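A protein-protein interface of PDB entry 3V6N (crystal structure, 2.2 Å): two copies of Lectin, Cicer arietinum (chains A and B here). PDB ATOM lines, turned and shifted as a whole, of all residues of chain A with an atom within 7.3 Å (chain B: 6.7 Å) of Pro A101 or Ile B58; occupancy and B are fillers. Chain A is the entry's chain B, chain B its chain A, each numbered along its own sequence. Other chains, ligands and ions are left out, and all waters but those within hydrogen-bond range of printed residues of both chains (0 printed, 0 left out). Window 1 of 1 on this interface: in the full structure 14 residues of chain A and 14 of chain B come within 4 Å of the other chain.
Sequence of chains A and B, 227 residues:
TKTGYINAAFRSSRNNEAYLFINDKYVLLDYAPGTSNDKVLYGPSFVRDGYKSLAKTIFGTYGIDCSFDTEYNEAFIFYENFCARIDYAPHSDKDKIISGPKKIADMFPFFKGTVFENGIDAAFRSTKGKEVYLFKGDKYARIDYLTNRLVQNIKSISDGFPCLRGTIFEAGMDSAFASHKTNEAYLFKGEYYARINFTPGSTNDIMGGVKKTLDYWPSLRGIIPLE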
ATOM      1  N   LYS A  56      29.956  -3.306  12.927  1.00  0.00           N
ATOM      2  CA  LYS A  56      30.016  -4.776  12.827  1.00  0.00           C
ATOM      3  C   LYS A  56      29.498  -5.305  11.481  1.00  0.00           C
ATOM      4  O   LYS A  56      28.627  -6.158  11.444  1.00  0.00           O
ATOM      5  CB  LYS A  56      29.287  -5.487  14.000  1.00  0.00           C
ATOM      6  CG  LYS A  56      29.156  -4.721  15.320  1.00  0.00           C
ATOM      7  CD  LYS A  56      30.481  -4.348  15.950  1.00  0.00           C
ATOM      8  CE  LYS A  56      31.325  -5.579  16.118  1.00  0.00           C
ATOM      9  NZ  LYS A  56      31.871  -6.098  14.853  1.00  0.00           N
ATOM     10  N   THR A  57      30.060  -4.791  10.389  1.00  0.00           N
ATOM     11  CA  THR A  57      29.740  -5.214   9.030  1.00  0.00           C
ATOM     12  C   THR A  57      31.059  -5.382   8.261  1.00  0.00           C
ATOM     13  O   THR A  57      32.100  -4.937   8.709  1.00  0.00           O
ATOM     14  CB  THR A  57      28.875  -4.175   8.260  1.00  0.00           C
ATOM     15  OG1 THR A  57      29.698  -3.067   7.879  1.00  0.00           O
ATOM     16  CG2 THR A  57      27.682  -3.674   9.090  1.00  0.00           C
ATOM     17  N   ILE A  58      30.995  -6.016   7.095  1.00  0.00           N
ATOM     18  CA  ILE A  58      32.165  -6.196   6.237  1.00  0.00           C
ATOM     19  C   ILE A  58      32.821  -4.867   5.858  1.00  0.00           C
ATOM     20  O   ILE A  58      34.039  -4.813   5.658  1.00  0.00           O
ATOM     21  CB  ILE A  58      31.795  -6.964   4.955  1.00  0.00           C
ATOM     22  CG1 ILE A  58      30.702  -6.213   4.186  1.00  0.00           C
ATOM     23  CG2 ILE A  58      31.379  -8.385   5.305  1.00  0.00           C
ATOM     24  CD1 ILE A  58      30.291  -6.850   2.877  1.00  0.00           C
ATOM     25  N   PHE A  59      32.017  -3.801   5.762  1.00  0.00           N
ATOM     26  CA  PHE A  59      32.545  -2.466   5.499  1.00  0.00           C
ATOM     27  C   PHE A  59      33.370  -1.939   6.664  1.00  0.00           C
ATOM     28  O   PHE A  59      34.374  -1.251   6.453  1.00  0.00           O
ATOM     29  CB  PHE A  59      31.424  -1.472   5.142  1.00  0.00           C
ATOM     30  CG  PHE A  59      30.441  -2.003   4.144  1.00  0.00           C
ATOM     31  CD1 PHE A  59      30.779  -2.107   2.791  1.00  0.00           C
ATOM     32  CD2 PHE A  59      29.177  -2.413   4.553  1.00  0.00           C
ATOM     33  CE1 PHE A  59      29.862  -2.597   1.870  1.00  0.00           C
ATOM     34  CE2 PHE A  59      28.258  -2.900   3.632  1.00  0.00           C
ATOM     35  CZ  PHE A  59      28.600  -2.995   2.285  1.00  0.00           C
ATOM     36  N   PHE A  82      29.667  -7.145  -2.596  1.00  0.00           N
ATOM     37  CA  PHE A  82      28.560  -6.738  -1.760  1.00  0.00           C
ATOM     38  C   PHE A  82      28.418  -5.231  -1.822  1.00  0.00           C
ATOM     39  O   PHE A  82      29.373  -4.543  -2.126  1.00  0.00           O
ATOM     40  CB  PHE A  82      28.778  -7.185  -0.308  1.00  0.00           C
ATOM     41  CG  PHE A  82      28.762  -8.672  -0.127  1.00  0.00           C
ATOM     42  CD1 PHE A  82      29.947  -9.407  -0.191  1.00  0.00           C
ATOM     43  CD2 PHE A  82      27.559  -9.347   0.065  1.00  0.00           C
ATOM     44  CE1 PHE A  82      29.938 -10.798  -0.052  1.00  0.00           C
ATOM     45  CE2 PHE A  82      27.545 -10.732   0.197  1.00  0.00           C
ATOM     46  CZ  PHE A  82      28.734 -11.458   0.142  1.00  0.00           C
ATOM     47  N   CYS A  83      27.215  -4.740  -1.541  1.00  0.00           N
ATOM     48  CA  CYS A  83      26.935  -3.312  -1.474  1.00  0.00           C
ATOM     49  C   CYS A  83      25.782  -3.017  -0.526  1.00  0.00           C
ATOM     50  O   CYS A  83      24.990  -3.893  -0.197  1.00  0.00           O
ATOM     51  CB  CYS A  83      26.608  -2.734  -2.856  1.00  0.00           C
ATOM     52  SG  CYS A  83      25.158  -3.461  -3.635  1.00  0.00           S
ATOM     53  N   ALA A  84      25.703  -1.765  -0.103  1.00  0.00           N
ATOM     54  CA  ALA A  84      24.682  -1.308   0.843  1.00  0.00           C
ATOM     55  C   ALA A  84      24.274   0.120   0.497  1.00  0.00           C
ATOM     56  O   ALA A  84      25.072   0.894  -0.039  1.00  0.00           O
ATOM     57  CB  ALA A  84      25.207  -1.370   2.268  1.00  0.00           C
ATOM     58  N   ARG A  85      23.023   0.446   0.782  1.00  0.00           N
ATOM     59  CA  ARG A  85      22.532   1.816   0.695  1.00  0.00           C
ATOM     60  C   ARG A  85      22.547   2.438   2.089  1.00  0.00           C
ATOM     61  O   ARG A  85      21.898   1.921   2.995  1.00  0.00           O
ATOM     62  CB  ARG A  85      21.119   1.803   0.112  1.00  0.00           C
ATOM     63  CG  ARG A  85      20.159   2.817   0.720  1.00  0.00           C
ATOM     64  CD  ARG A  85      19.420   3.580  -0.352  1.00  0.00           C
ATOM     65  NE  ARG A  85      20.287   4.675  -0.757  1.00  0.00           N
ATOM     66  CZ  ARG A  85      21.421   4.518  -1.421  1.00  0.00           C
ATOM     67  NH1 ARG A  85      21.821   3.322  -1.764  1.00  0.00           N
ATOM     68  NH2 ARG A  85      22.164   5.560  -1.745  1.00  0.00           N
ATOM     69  N   ILE A  97      22.179   2.139   7.897  1.00  0.00           N
ATOM     70  CA  ILE A  97      22.038   1.367   6.681  1.00  0.00           C
ATOM     71  C   ILE A  97      20.554   1.321   6.363  1.00  0.00           C
ATOM     72  O   ILE A  97      19.755   0.943   7.212  1.00  0.00           O
ATOM     73  CB  ILE A  97      22.577  -0.060   6.867  1.00  0.00           C
ATOM     74  CG1 ILE A  97      24.081  -0.005   7.179  1.00  0.00           C
ATOM     75  CG2 ILE A  97      22.254  -0.917   5.641  1.00  0.00           C
ATOM     76  CD1 ILE A  97      24.697  -1.328   7.600  1.00  0.00           C
ATOM     77  N   SER A  99      19.408  -0.123   3.158  1.00  0.00           N
ATOM     78  CA  SER A  99      19.199  -1.339   2.359  1.00  0.00           C
ATOM     79  C   SER A  99      20.475  -2.151   2.339  1.00  0.00           C
ATOM     80  O   SER A  99      21.543  -1.597   2.116  1.00  0.00           O
ATOM     81  CB  SER A  99      18.853  -0.995   0.911  1.00  0.00           C
ATOM     82  OG  SER A  99      17.466  -0.964   0.703  1.00  0.00           O
ATOM     83  N   GLY A 100      20.356  -3.457   2.564  1.00  0.00           N
ATOM     84  CA  GLY A 100      21.489  -4.371   2.505  1.00  0.00           C
ATOM     85  C   GLY A 100      22.157  -4.664   3.836  1.00  0.00           C
ATOM     86  O   GLY A 100      21.581  -4.388   4.884  1.00  0.00           O
ATOM     87  N   PRO A 101      23.384  -5.221   3.802  1.00  0.00           N
ATOM     88  CA  PRO A 101      24.161  -5.485   2.582  1.00  0.00           C
ATOM     89  C   PRO A 101      23.560  -6.594   1.722  1.00  0.00           C
ATOM     90  O   PRO A 101      23.010  -7.560   2.257  1.00  0.00           O
ATOM     91  CB  PRO A 101      25.541  -5.928   3.106  1.00  0.00           C
ATOM     92  CG  PRO A 101      25.468  -5.852   4.604  1.00  0.00           C
ATOM     93  CD  PRO A 101      24.023  -5.803   4.990  1.00  0.00           C
ATOM     94  N   LYS A 102      23.661  -6.426   0.405  1.00  0.00           N
ATOM     95  CA  LYS A 102      23.197  -7.386  -0.588  1.00  0.00           C
ATOM     96  C   LYS A 102      24.328  -7.593  -1.577  1.00  0.00           C
ATOM     97  O   LYS A 102      25.180  -6.716  -1.740  1.00  0.00           O
ATOM     98  CB  LYS A 102      22.017  -6.819  -1.376  1.00  0.00           C
ATOM     99  CG  LYS A 102      20.665  -6.861  -0.681  1.00  0.00           C
ATOM    100  CD  LYS A 102      19.542  -6.788  -1.714  1.00  0.00           C
ATOM    101  CE  LYS A 102      18.295  -6.128  -1.155  1.00  0.00           C
ATOM    102  NZ  LYS A 102      17.717  -6.944  -0.053  1.00  0.00           N
ATOM    103  N   LYS A 103      24.327  -8.735  -2.262  1.00  0.00           N
ATOM    104  CA  LYS A 103      25.232  -8.939  -3.386  1.00  0.00           C
ATOM    105  C   LYS A 103      24.893  -7.955  -4.517  1.00  0.00           C
ATOM    106  O   LYS A 103      23.732  -7.546  -4.676  1.00  0.00           O
ATOM    107  CB  LYS A 103      25.154 -10.382  -3.881  1.00  0.00           C
ATOM    108  CG  LYS A 103      25.575 -11.428  -2.854  1.00  0.00           C
ATOM    109  CD  LYS A 103      25.380 -12.845  -3.381  1.00  0.00           C
ATOM    110  CE  LYS A 103      25.914 -13.842  -2.365  1.00  0.00           C
ATOM    111  NZ  LYS A 103      25.854 -15.253  -2.828  1.00  0.00           N
ATOM    112  N   MET A 107      21.140  -6.431  -6.001  1.00  0.00           N
ATOM    113  CA  MET A 107      20.790  -5.009  -6.017  1.00  0.00           C
ATOM    114  C   MET A 107      20.635  -4.456  -7.447  1.00  0.00           C
ATOM    115  O   MET A 107      19.742  -3.659  -7.723  1.00  0.00           O
ATOM    116  CB  MET A 107      21.850  -4.216  -5.259  1.00  0.00           C
ATOM    117  CG  MET A 107      21.454  -2.785  -4.961  1.00  0.00           C
ATOM    118  SD  MET A 107      20.437  -2.661  -3.481  1.00  0.00           S
ATOM    119  CE  MET A 107      21.708  -2.831  -2.219  1.00  0.00           C
ATOM    120  N   LEU B  54      21.924  -8.795  13.947  1.00  0.00           N
ATOM    121  CA  LEU B  54      22.274  -9.325  12.635  1.00  0.00           C
ATOM    122  C   LEU B  54      21.475  -8.707  11.496  1.00  0.00           C
ATOM    123  O   LEU B  54      21.751  -8.989  10.338  1.00  0.00           O
ATOM    124  CB  LEU B  54      22.175 -10.870  12.591  1.00  0.00           C
ATOM    125  CG  LEU B  54      23.031 -11.714  13.542  1.00  0.00           C
ATOM    126  CD1 LEU B  54      22.873 -13.217  13.303  1.00  0.00           C
ATOM    127  CD2 LEU B  54      24.498 -11.316  13.469  1.00  0.00           C
ATOM    128  N   ALA B  55      20.528  -7.830  11.836  1.00  0.00           N
ATOM    129  CA  ALA B  55      19.560  -7.291  10.884  1.00  0.00           C
ATOM    130  C   ALA B  55      20.163  -6.644   9.649  1.00  0.00           C
ATOM    131  O   ALA B  55      19.649  -6.842   8.558  1.00  0.00           O
ATOM    132  CB  ALA B  55      18.595  -6.306  11.570  1.00  0.00           C
ATOM    133  N   LYS B  56      21.197  -5.830   9.808  1.00  0.00           N
ATOM    134  CA  LYS B  56      21.788  -5.168   8.636  1.00  0.00           C
ATOM    135  C   LYS B  56      23.181  -5.737   8.332  1.00  0.00           C
ATOM    136  O   LYS B  56      24.137  -4.980   8.203  1.00  0.00           O
ATOM    137  CB  LYS B  56      21.856  -3.622   8.826  1.00  0.00           C
ATOM    138  CG  LYS B  56      20.593  -2.926   9.359  1.00  0.00           C
ATOM    139  CD  LYS B  56      19.364  -3.234   8.549  1.00  0.00           C
ATOM    140  CE  LYS B  56      19.567  -2.818   7.107  1.00  0.00           C
ATOM    141  NZ  LYS B  56      19.348  -3.942   6.162  1.00  0.00           N
ATOM    142  N   THR B  57      23.290  -7.071   8.269  1.00  0.00           N
ATOM    143  CA  THR B  57      24.542  -7.762   7.947  1.00  0.00           C
ATOM    144  C   THR B  57      24.250  -8.786   6.848  1.00  0.00           C
ATOM    145  O   THR B  57      23.084  -9.051   6.530  1.00  0.00           O
ATOM    146  CB  THR B  57      25.200  -8.485   9.173  1.00  0.00           C
ATOM    147  OG1 THR B  57      24.399  -9.599   9.583  1.00  0.00           O
ATOM    148  CG2 THR B  57      25.434  -7.538  10.374  1.00  0.00           C
ATOM    149  N   ILE B  58      25.303  -9.361   6.267  1.00  0.00           N
ATOM    150  CA  ILE B  58      25.128 -10.433   5.275  1.00  0.00           C
ATOM    151  C   ILE B  58      24.387 -11.645   5.848  1.00  0.00           C
ATOM    152  O   ILE B  58      23.702 -12.357   5.123  1.00  0.00           O
ATOM    153  CB  ILE B  58      26.476 -10.884   4.686  1.00  0.00           C
ATOM    154  CG1 ILE B  58      27.371 -11.443   5.801  1.00  0.00           C
ATOM    155  CG2 ILE B  58      27.093  -9.724   3.899  1.00  0.00           C
ATOM    156  CD1 ILE B  58      28.810 -11.709   5.427  1.00  0.00           C
ATOM    157  N   PHE B  59      24.530 -11.869   7.151  1.00  0.00           N
ATOM    158  CA  PHE B  59      23.788 -12.942   7.837  1.00  0.00           C
ATOM    159  C   PHE B  59      22.290 -12.647   7.841  1.00  0.00           C
ATOM    160  O   PHE B  59      21.486 -13.533   7.580  1.00  0.00           O
ATOM    161  CB  PHE B  59      24.331 -13.159   9.250  1.00  0.00           C
ATOM    162  CG  PHE B  59      25.818 -13.304   9.293  1.00  0.00           C
ATOM    163  CD1 PHE B  59      26.431 -14.471   8.843  1.00  0.00           C
ATOM    164  CD2 PHE B  59      26.619 -12.271   9.754  1.00  0.00           C
ATOM    165  CE1 PHE B  59      27.806 -14.609   8.871  1.00  0.00           C
ATOM    166  CE2 PHE B  59      28.006 -12.410   9.777  1.00  0.00           C
ATOM    167  CZ  PHE B  59      28.599 -13.578   9.338  1.00  0.00           C
ATOM    168  N   GLY B  60      21.930 -11.385   8.097  1.00  0.00           N
ATOM    169  CA  GLY B  60      20.525 -10.967   8.128  1.00  0.00           C
ATOM    170  C   GLY B  60      19.921 -11.041   6.738  1.00  0.00           C
ATOM    171  O   GLY B  60      18.772 -11.412   6.581  1.00  0.00           O
ATOM    172  N   THR B  61      20.700 -10.682   5.721  1.00  0.00           N
ATOM    173  CA  THR B  61      20.231 -10.763   4.346  1.00  0.00           C
ATOM    174  C   THR B  61      20.107 -12.225   3.865  1.00  0.00           C
ATOM    175  O   THR B  61      19.054 -12.607   3.388  1.00  0.00           O
ATOM    176  CB  THR B  61      21.131  -9.960   3.392  1.00  0.00           C
ATOM    177  OG1 THR B  61      21.222  -8.606   3.855  1.00  0.00           O
ATOM    178  CG2 THR B  61      20.558  -9.971   1.955  1.00  0.00           C
ATOM    179  N   TYR B  62      21.175 -13.023   3.998  1.00  0.00           N
ATOM    180  CA  TYR B  62      21.239 -14.348   3.336  1.00  0.00           C
ATOM    181  C   TYR B  62      21.152 -15.554   4.265  1.00  0.00           C
ATOM    182  O   TYR B  62      21.062 -16.694   3.785  1.00  0.00           O
ATOM    183  CB  TYR B  62      22.472 -14.462   2.429  1.00  0.00           C
ATOM    184  CG  TYR B  62      22.460 -13.435   1.321  1.00  0.00           C
ATOM    185  CD1 TYR B  62      21.588 -13.571   0.245  1.00  0.00           C
ATOM    186  CD2 TYR B  62      23.300 -12.320   1.360  1.00  0.00           C
ATOM    187  CE1 TYR B  62      21.534 -12.625  -0.759  1.00  0.00           C
ATOM    188  CE2 TYR B  62      23.285 -11.375   0.339  1.00  0.00           C
ATOM    189  CZ  TYR B  62      22.388 -11.525  -0.713  1.00  0.00           C
ATOM    190  OH  TYR B  62      22.337 -10.593  -1.731  1.00  0.00           O
ATOM    191  N   GLY B  63      21.169 -15.310   5.575  1.00  0.00           N
ATOM    192  CA  GLY B  63      21.125 -16.387   6.558  1.00  0.00           C
ATOM    193  C   GLY B  63      22.479 -16.985   6.907  1.00  0.00           C
ATOM    194  O   GLY B  63      23.543 -16.412   6.608  1.00  0.00           O
ATOM    195  N   ILE B  64      22.435 -18.157   7.525  1.00  0.00           N
ATOM    196  CA  ILE B  64      23.619 -18.788   8.107  1.00  0.00           C
ATOM    197  C   ILE B  64      23.788 -20.193   7.533  1.00  0.00           C
ATOM    198  O   ILE B  64      22.824 -20.986   7.538  1.00  0.00           O
ATOM    199  CB  ILE B  64      23.493 -18.799   9.649  1.00  0.00           C
ATOM    200  CG1 ILE B  64      23.594 -17.349  10.165  1.00  0.00           C
ATOM    201  CG2 ILE B  64      24.538 -19.706  10.298  1.00  0.00           C
ATOM    202  CD1 ILE B  64      23.055 -17.112  11.564  1.00  0.00           C
ATOM    203  N   TYR B  79      28.711 -17.456   6.748  1.00  0.00           N
ATOM    204  CA  TYR B  79      28.019 -17.375   5.470  1.00  0.00           C
ATOM    205  C   TYR B  79      29.060 -17.281   4.348  1.00  0.00           C
ATOM    206  O   TYR B  79      29.876 -16.334   4.314  1.00  0.00           O
ATOM    207  CB  TYR B  79      27.043 -16.197   5.396  1.00  0.00           C
ATOM    208  CG  TYR B  79      26.442 -16.096   4.001  1.00  0.00           C
ATOM    209  CD1 TYR B  79      25.496 -17.026   3.572  1.00  0.00           C
ATOM    210  CD2 TYR B  79      26.855 -15.108   3.101  1.00  0.00           C
ATOM    211  CE1 TYR B  79      24.961 -16.970   2.304  1.00  0.00           C
ATOM    212  CE2 TYR B  79      26.315 -15.038   1.822  1.00  0.00           C
ATOM    213  CZ  TYR B  79      25.365 -15.969   1.433  1.00  0.00           C
ATOM    214  OH  TYR B  79      24.821 -15.934   0.163  1.00  0.00           O
ATOM    215  N   PHE B  82      32.677 -15.783   4.902  1.00  0.00           N
ATOM    216  CA  PHE B  82      32.695 -14.879   6.061  1.00  0.00           C
ATOM    217  C   PHE B  82      32.198 -15.558   7.329  1.00  0.00           C
ATOM    218  O   PHE B  82      31.368 -16.450   7.268  1.00  0.00           O
ATOM    219  CB  PHE B  82      31.850 -13.628   5.785  1.00  0.00           C
ATOM    220  CG  PHE B  82      32.361 -12.801   4.641  1.00  0.00           C
ATOM    221  CD1 PHE B  82      31.868 -12.989   3.353  1.00  0.00           C
ATOM    222  CD2 PHE B  82      33.365 -11.858   4.841  1.00  0.00           C
ATOM    223  CE1 PHE B  82      32.354 -12.234   2.289  1.00  0.00           C
ATOM    224  CE2 PHE B  82      33.846 -11.108   3.785  1.00  0.00           C
ATOM    225  CZ  PHE B  82      33.341 -11.302   2.506  1.00  0.00           C
ATOM    226  N   CYS B  83      32.711 -15.123   8.477  1.00  0.00           N
ATOM    227  CA  CYS B  83      32.259 -15.630   9.756  1.00  0.00           C
ATOM    228  C   CYS B  83      32.216 -14.539  10.828  1.00  0.00           C
ATOM    229  O   CYS B  83      32.789 -13.460  10.659  1.00  0.00           O
ATOM    230  CB  CYS B  83      33.142 -16.797  10.217  1.00  0.00           C
ATOM    231  SG  CYS B  83      34.881 -16.387  10.376  1.00  0.00           S
ATOM    232  N   PRO B 101      32.078  -9.100  11.119  1.00  0.00           N
ATOM    233  CA  PRO B 101      32.454 -10.273  10.310  1.00  0.00           C
ATOM    234  C   PRO B 101      33.886 -10.210   9.784  1.00  0.00           C
ATOM    235  O   PRO B 101      34.399  -9.124   9.536  1.00  0.00           O
ATOM    236  CB  PRO B 101      31.457 -10.257   9.134  1.00  0.00           C
ATOM    237  CG  PRO B 101      30.546  -9.096   9.365  1.00  0.00           C
ATOM    238  CD  PRO B 101      31.155  -8.205  10.411  1.00  0.00           C
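Of the 15 printed residues of chain A, 9 touch a printed residue of chain B.
Hydrophobic or aromatic side chains of chain A that line the printed part of chain B: Ile A58, Phe A82, Ile A97 and Pro A101.
Among the printed residues, 17 pairs touch across the chains.
CG2 of Thr B57 touches O of Lys A56, at 3.6 Å.
Pro B101 touches Lys A56 (CD to O, 3.4 Å).
C of Thr A57 touches CD of Pro B101 (3.5 Å).
CE2 of Phe B82 touches CG2 of Ile A58 (3.98 Å).
N of Ile A58 touches CG of Pro B101, 3.9 Å away.
Phe A82 touches Ile B58.
Phe B82 touches Phe A82.
CE of Lys B56 touches CG2 of Ile A97, at 3.6 Å.
Pro A101 touches Lys B56 (CD to O, 3.3 Å).
Pro A101 touches Thr B57.
The backbone carbonyl oxygen (O) of Leu B54 is in hydrogen-bond range of the side-chain hydroxyl (OG1) of Thr B57 (2.8 Å).
OG1 of Thr B57 lies close to N of Phe B59 (3.3 Å).
The side-chain hydroxyl (OG1) of Thr B57 is in hydrogen-bond range of the backbone NH (N) of Gly B60 (3.4 Å).
O of Thr B57 sits at hydrogen-bond distance from OG1 of Thr B61, 3.3 Å away.
The backbone NH (N) of Phe A59 lies close to the side-chain hydroxyl (OG1) of Thr A57 (3.2 Å).
N of Cys A83 lies within hydrogen-bond range of O of Lys A102 (2.8 Å).
NZ of Lys B56 is in hydrogen-bond range of O of Gly A100, at 2.6 Å.
OG1 of Thr B61 lies within hydrogen-bond range of O of Pro A101.
N of Lys A103 is in hydrogen-bond range of OH of Tyr B62 (2.8 Å).
The side-chain hydroxyl (OH) of Tyr B79 lies within hydrogen-bond range of the side-chain amino group (NZ) of Lys A103 (3.2 Å).
Printed residues of chain B within 4 Å of Ile A58: Phe B82 (3.98 Å) and Pro B101 (3.9 Å).
Ile B58 touches just these residues of chain A: Phe A82 and Pro A101.
Of the printed residues of chain A, Tyr B62 touches Lys A102 and Lys A103.
The nearest residue of chain B that does not touch Pro A101 is Tyr B62 (4.3 Å).
Lys A56 touches Pro B101, and with the chains exchanged Pro A101 touches Lys B56.
Thr A57 touches Pro B101, and with the chains exchanged Pro A101 touches Thr B57.
Ile A58 touches Phe B82, and with the chains exchanged Phe A82 touches Ile B58.
Phe B82 touches its own counterpart, Phe A82.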
